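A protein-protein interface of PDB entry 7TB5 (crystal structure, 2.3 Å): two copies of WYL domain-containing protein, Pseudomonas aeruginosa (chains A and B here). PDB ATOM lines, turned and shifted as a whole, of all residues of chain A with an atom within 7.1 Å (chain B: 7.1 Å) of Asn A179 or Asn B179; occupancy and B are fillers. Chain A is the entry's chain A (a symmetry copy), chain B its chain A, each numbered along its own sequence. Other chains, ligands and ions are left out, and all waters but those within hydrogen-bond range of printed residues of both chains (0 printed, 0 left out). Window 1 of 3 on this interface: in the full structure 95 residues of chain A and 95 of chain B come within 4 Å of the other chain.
The indole nitrogen of Trp A181 sits at hydrogen-bond distance from the side-chain carboxylate of Asp B101 (3.2 Å).
The side-chain amide nitrogen (ND2) of Asn A179 lies close to the side-chain amide nitrogen (ND2) of Asn B179.
The indole nitrogen of Trp B181 sits at hydrogen-bond distance from the side-chain carboxylate of Asp A101.
Among the printed residues, pairs that only touch across the chains: Gly A178 with Asn B179 (3.5 Å), Asn A179 with Gly B178 (3.5 Å), Asp A101 with Leu B134 (3.9 Å) and Leu A134 with Asp B101 (3.9 Å).
Of the printed residues of chain B, Asp A101 touches Leu B134 (3.9 Å) and Trp B181 (3.2 Å).
Of the printed residues of chain B, Gly A178 touches Asn B179 (3.5 Å).
Asn A179 touches just these residues of chain B: Gly B178 and Asn B179.
Pro A280 touches none of the printed residues of chain B.
Asn B179 touches just these residues of chain A: Gly A178 (3.5 Å) and Asn A179 (3.4 Å).
The nearest printed residue of chain A that does not touch Trp B181 is Asn A179 (9.9 Å).
Of the 9 printed residues of chain A, 5 touch a printed residue of chain B.
Hydrophobic or aromatic side chains of chain A within 4 Å of the printed part of chain B: Leu A134 and Trp A181.
Asp A101 touches Leu B134, and with the chains exchanged Leu A134 touches Asp B101.
Asp A101 touches Trp B181, and with the chains exchanged Trp A181 touches Asp B101.
Gly A178 touches Asn B179, and with the chains exchanged Asn A179 touches Gly B178.
Asn A179 touches its own counterpart, Asn B179.
Of the 7 pairs that touch across the chains among the printed residues, 7 have their exchanged pair printed and touching as well.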
ATOM      1  N   ASP A 101     -16.067  -6.563  27.523  1.00  0.00           N
ATOM      2  CA  ASP A 101     -16.203  -5.461  26.570  1.00  0.00           C
ATOM      3  C   ASP A 101     -16.024  -5.962  25.145  1.00  0.00           C
ATOM      4  O   ASP A 101     -16.696  -5.485  24.225  1.00  0.00           O
ATOM      5  CB  ASP A 101     -15.195  -4.340  26.853  1.00  0.00           C
ATOM      6  CG  ASP A 101     -15.228  -3.881  28.295  1.00  0.00           C
ATOM      7  OD1 ASP A 101     -15.287  -4.748  29.208  1.00  0.00           O
ATOM      8  OD2 ASP A 101     -15.215  -2.651  28.516  1.00  0.00           O
ATOM      9  N   LEU A 134      -3.209   0.397  15.348  1.00  0.00           N
ATOM     10  CA  LEU A 134      -2.084  -0.432  15.744  1.00  0.00           C
ATOM     11  C   LEU A 134      -1.561  -1.215  14.554  1.00  0.00           C
ATOM     12  O   LEU A 134      -2.341  -1.760  13.772  1.00  0.00           O
ATOM     13  CB  LEU A 134      -2.546  -1.383  16.830  1.00  0.00           C
ATOM     14  CG  LEU A 134      -1.502  -1.948  17.780  1.00  0.00           C
ATOM     15  CD1 LEU A 134      -0.747  -0.892  18.534  1.00  0.00           C
ATOM     16  CD2 LEU A 134      -2.240  -2.898  18.764  1.00  0.00           C
ATOM     17  N   HIS A 176      -0.160  -2.517  28.039  1.00  0.00           N
ATOM     18  CA  HIS A 176      -1.477  -1.982  27.714  1.00  0.00           C
ATOM     19  C   HIS A 176      -1.836  -0.918  28.734  1.00  0.00           C
ATOM     20  O   HIS A 176      -1.808  -1.173  29.942  1.00  0.00           O
ATOM     21  CB  HIS A 176      -2.516  -3.102  27.759  1.00  0.00           C
ATOM     22  CG  HIS A 176      -3.814  -2.777  27.082  1.00  0.00           C
ATOM     23  ND1 HIS A 176      -5.017  -3.355  27.445  1.00  0.00           N
ATOM     24  CD2 HIS A 176      -4.096  -1.943  26.052  1.00  0.00           C
ATOM     25  CE1 HIS A 176      -5.979  -2.882  26.671  1.00  0.00           C
ATOM     26  NE2 HIS A 176      -5.449  -2.017  25.825  1.00  0.00           N
ATOM     27  N   ASP A 177      -2.147   0.273  28.254  1.00  0.00           N
ATOM     28  CA  ASP A 177      -2.638   1.359  29.102  1.00  0.00           C
ATOM     29  C   ASP A 177      -4.009   1.813  28.591  1.00  0.00           C
ATOM     30  O   ASP A 177      -4.123   2.832  27.900  1.00  0.00           O
ATOM     31  CB  ASP A 177      -1.639   2.511  29.092  1.00  0.00           C
ATOM     32  CG  ASP A 177      -2.157   3.740  29.827  1.00  0.00           C
ATOM     33  OD1 ASP A 177      -3.142   3.618  30.606  1.00  0.00           O
ATOM     34  OD2 ASP A 177      -1.571   4.826  29.611  1.00  0.00           O
ATOM     35  N   GLY A 178      -5.043   1.063  28.943  1.00  0.00           N
ATOM     36  CA  GLY A 178      -6.362   1.298  28.389  1.00  0.00           C
ATOM     37  C   GLY A 178      -6.332   1.233  26.889  1.00  0.00           C
ATOM     38  O   GLY A 178      -6.153   0.144  26.355  1.00  0.00           O
ATOM     39  N   ASN A 179      -6.491   2.363  26.194  1.00  0.00           N
ATOM     40  CA  ASN A 179      -6.382   2.357  24.734  1.00  0.00           C
ATOM     41  C   ASN A 179      -4.938   2.215  24.239  1.00  0.00           C
ATOM     42  O   ASN A 179      -4.692   1.535  23.236  1.00  0.00           O
ATOM     43  CB  ASN A 179      -7.007   3.637  24.182  1.00  0.00           C
ATOM     44  CG  ASN A 179      -8.270   4.041  24.940  1.00  0.00           C
ATOM     45  OD1 ASN A 179      -9.336   3.424  24.788  1.00  0.00           O
ATOM     46  ND2 ASN A 179      -8.153   5.083  25.757  1.00  0.00           N
ATOM     47  N   ARG A 180      -3.975   2.826  24.919  1.00  0.00           N
ATOM     48  CA  ARG A 180      -2.629   2.977  24.387  1.00  0.00           C
ATOM     49  C   ARG A 180      -1.716   1.811  24.761  1.00  0.00           C
ATOM     50  O   ARG A 180      -1.772   1.256  25.862  1.00  0.00           O
ATOM     51  CB  ARG A 180      -2.010   4.280  24.893  1.00  0.00           C
ATOM     52  CG  ARG A 180      -2.708   5.540  24.385  1.00  0.00           C
ATOM     53  CD  ARG A 180      -2.757   5.529  22.858  1.00  0.00           C
ATOM     54  NE  ARG A 180      -3.684   6.534  22.347  1.00  0.00           N
ATOM     55  CZ  ARG A 180      -4.267   6.479  21.154  1.00  0.00           C
ATOM     56  NH1 ARG A 180      -4.023   5.479  20.317  1.00  0.00           N
ATOM     57  NH2 ARG A 180      -5.105   7.456  20.788  1.00  0.00           N
ATOM     58  N   TRP A 181      -0.840   1.475  23.829  1.00  0.00           N
ATOM     59  CA  TRP A 181       0.226   0.505  24.026  1.00  0.00           C
ATOM     60  C   TRP A 181       1.583   1.200  24.030  1.00  0.00           C
ATOM     61  O   TRP A 181       1.804   2.193  23.329  1.00  0.00           O
ATOM     62  CB  TRP A 181       0.211  -0.534  22.912  1.00  0.00           C
ATOM     63  CG  TRP A 181      -0.953  -1.456  22.943  1.00  0.00           C
ATOM     64  CD1 TRP A 181      -2.163  -1.311  22.285  1.00  0.00           C
ATOM     65  CD2 TRP A 181      -1.039  -2.683  23.667  1.00  0.00           C
ATOM     66  NE1 TRP A 181      -2.977  -2.375  22.573  1.00  0.00           N
ATOM     67  CE2 TRP A 181      -2.316  -3.225  23.420  1.00  0.00           C
ATOM     68  CE3 TRP A 181      -0.173  -3.363  24.520  1.00  0.00           C
ATOM     69  CZ2 TRP A 181      -2.719  -4.425  23.956  1.00  0.00           C
ATOM     70  CZ3 TRP A 181      -0.584  -4.541  25.058  1.00  0.00           C
ATOM     71  CH2 TRP A 181      -1.849  -5.056  24.793  1.00  0.00           C
ATOM     72  N   PRO A 280      -1.551  10.783  23.814  1.00  0.00           N
ATOM     73  CA  PRO A 280      -1.725  10.582  22.366  1.00  0.00           C
ATOM     74  C   PRO A 280      -1.430  11.841  21.565  1.00  0.00           C
ATOM     75  O   PRO A 280      -1.603  12.966  22.045  1.00  0.00           O
ATOM     76  CB  PRO A 280      -3.198  10.169  22.233  1.00  0.00           C
ATOM     77  CG  PRO A 280      -3.567   9.609  23.606  1.00  0.00           C
ATOM     78  CD  PRO A 280      -2.767  10.449  24.581  1.00  0.00           C
ATOM     79  N   ASP B 101      -6.057  -5.524  19.298  1.00  0.00           N
ATOM     80  CA  ASP B 101      -5.694  -5.299  20.695  1.00  0.00           C
ATOM     81  C   ASP B 101      -6.159  -6.459  21.563  1.00  0.00           C
ATOM     82  O   ASP B 101      -5.471  -6.845  22.513  1.00  0.00           O
ATOM     83  CB  ASP B 101      -6.283  -3.987  21.230  1.00  0.00           C
ATOM     84  CG  ASP B 101      -5.966  -2.805  20.341  1.00  0.00           C
ATOM     85  OD1 ASP B 101      -6.079  -2.936  19.092  1.00  0.00           O
ATOM     86  OD2 ASP B 101      -5.585  -1.748  20.889  1.00  0.00           O
ATOM     87  N   LEU B 134     -17.381  -3.584  34.464  1.00  0.00           N
ATOM     88  CA  LEU B 134     -18.658  -3.633  33.773  1.00  0.00           C
ATOM     89  C   LEU B 134     -19.511  -4.763  34.319  1.00  0.00           C
ATOM     90  O   LEU B 134     -19.015  -5.868  34.547  1.00  0.00           O
ATOM     91  CB  LEU B 134     -18.397  -3.848  32.295  1.00  0.00           C
ATOM     92  CG  LEU B 134     -19.461  -3.397  31.305  1.00  0.00           C
ATOM     93  CD1 LEU B 134     -19.781  -1.934  31.399  1.00  0.00           C
ATOM     94  CD2 LEU B 134     -18.947  -3.754  29.884  1.00  0.00           C
ATOM     95  N   HIS B 176     -19.863   2.618  22.878  1.00  0.00           N
ATOM     96  CA  HIS B 176     -18.485   2.431  23.319  1.00  0.00           C
ATOM     97  C   HIS B 176     -17.721   3.720  23.091  1.00  0.00           C
ATOM     98  O   HIS B 176     -17.701   4.249  21.976  1.00  0.00           O
ATOM     99  CB  HIS B 176     -17.834   1.303  22.519  1.00  0.00           C
ATOM    100  CG  HIS B 176     -16.574   0.756  23.122  1.00  0.00           C
ATOM    101  ND1 HIS B 176     -15.573   0.173  22.368  1.00  0.00           N
ATOM    102  CD2 HIS B 176     -16.161   0.691  24.410  1.00  0.00           C
ATOM    103  CE1 HIS B 176     -14.596  -0.219  23.169  1.00  0.00           C
ATOM    104  NE2 HIS B 176     -14.923   0.094  24.412  1.00  0.00           N
ATOM    105  N   ASP B 177     -17.115   4.237  24.146  1.00  0.00           N
ATOM    106  CA  ASP B 177     -16.236   5.402  24.055  1.00  0.00           C
ATOM    107  C   ASP B 177     -14.851   5.028  24.592  1.00  0.00           C
ATOM    108  O   ASP B 177     -14.505   5.351  25.735  1.00  0.00           O
ATOM    109  CB  ASP B 177     -16.836   6.562  24.843  1.00  0.00           C
ATOM    110  CG  ASP B 177     -15.899   7.759  24.923  1.00  0.00           C
ATOM    111  OD1 ASP B 177     -14.923   7.829  24.126  1.00  0.00           O
ATOM    112  OD2 ASP B 177     -16.148   8.624  25.794  1.00  0.00           O
ATOM    113  N   GLY B 178     -14.061   4.360  23.763  1.00  0.00           N
ATOM    114  CA  GLY B 178     -12.797   3.813  24.212  1.00  0.00           C
ATOM    115  C   GLY B 178     -12.997   2.890  25.381  1.00  0.00           C
ATOM    116  O   GLY B 178     -13.550   1.813  25.187  1.00  0.00           O
ATOM    117  N   ASN B 179     -12.575   3.281  26.588  1.00  0.00           N
ATOM    118  CA  ASN B 179     -12.829   2.450  27.766  1.00  0.00           C
ATOM    119  C   ASN B 179     -14.291   2.488  28.227  1.00  0.00           C
ATOM    120  O   ASN B 179     -14.831   1.462  28.656  1.00  0.00           O
ATOM    121  CB  ASN B 179     -11.906   2.896  28.898  1.00  0.00           C
ATOM    122  CG  ASN B 179     -10.510   3.264  28.399  1.00  0.00           C
ATOM    123  OD1 ASN B 179      -9.701   2.390  28.051  1.00  0.00           O
ATOM    124  ND2 ASN B 179     -10.223   4.561  28.369  1.00  0.00           N
ATOM    125  N   ARG B 180     -14.950   3.638  28.138  1.00  0.00           N
ATOM    126  CA  ARG B 180     -16.235   3.845  28.789  1.00  0.00           C
ATOM    127  C   ARG B 180     -17.414   3.465  27.897  1.00  0.00           C
ATOM    128  O   ARG B 180     -17.417   3.681  26.681  1.00  0.00           O
ATOM    129  CB  ARG B 180     -16.376   5.306  29.213  1.00  0.00           C
ATOM    130  CG  ARG B 180     -15.386   5.741  30.291  1.00  0.00           C
ATOM    131  CD  ARG B 180     -15.497   4.820  31.505  1.00  0.00           C
ATOM    132  NE  ARG B 180     -14.367   4.993  32.412  1.00  0.00           N
ATOM    133  CZ  ARG B 180     -13.953   4.074  33.276  1.00  0.00           C
ATOM    134  NH1 ARG B 180     -14.571   2.905  33.385  1.00  0.00           N
ATOM    135  NH2 ARG B 180     -12.900   4.339  34.061  1.00  0.00           N
ATOM    136  N   TRP B 181     -18.441   2.930  28.535  1.00  0.00           N
ATOM    137  CA  TRP B 181     -19.724   2.638  27.915  1.00  0.00           C
ATOM    138  C   TRP B 181     -20.800   3.573  28.458  1.00  0.00           C
ATOM    139  O   TRP B 181     -20.781   3.972  29.628  1.00  0.00           O
ATOM    140  CB  TRP B 181     -20.136   1.201  28.195  1.00  0.00           C
ATOM    141  CG  TRP B 181     -19.308   0.175  27.510  1.00  0.00           C
ATOM    142  CD1 TRP B 181     -18.185  -0.468  28.000  1.00  0.00           C
ATOM    143  CD2 TRP B 181     -19.523  -0.345  26.199  1.00  0.00           C
ATOM    144  NE1 TRP B 181     -17.705  -1.343  27.060  1.00  0.00           N
ATOM    145  CE2 TRP B 181     -18.502  -1.282  25.948  1.00  0.00           C
ATOM    146  CE3 TRP B 181     -20.464  -0.092  25.202  1.00  0.00           C
ATOM    147  CZ2 TRP B 181     -18.427  -1.989  24.772  1.00  0.00           C
ATOM    148  CZ3 TRP B 181     -20.374  -0.782  24.036  1.00  0.00           C
ATOM    149  CH2 TRP B 181     -19.357  -1.708  23.817  1.00  0.00           C
ATOM    150  N   PRO B 280     -14.958   9.687  33.952  1.00  0.00           N
ATOM    151  CA  PRO B 280     -15.000   8.632  34.977  1.00  0.00           C
ATOM    152  C   PRO B 280     -14.981   9.195  36.391  1.00  0.00           C
ATOM    153  O   PRO B 280     -14.429  10.269  36.649  1.00  0.00           O
ATOM    154  CB  PRO B 280     -13.742   7.800  34.691  1.00  0.00           C
ATOM    155  CG  PRO B 280     -13.422   8.076  33.223  1.00  0.00           C
ATOM    156  CD  PRO B 280     -13.827   9.521  33.016  1.00  0.00           C
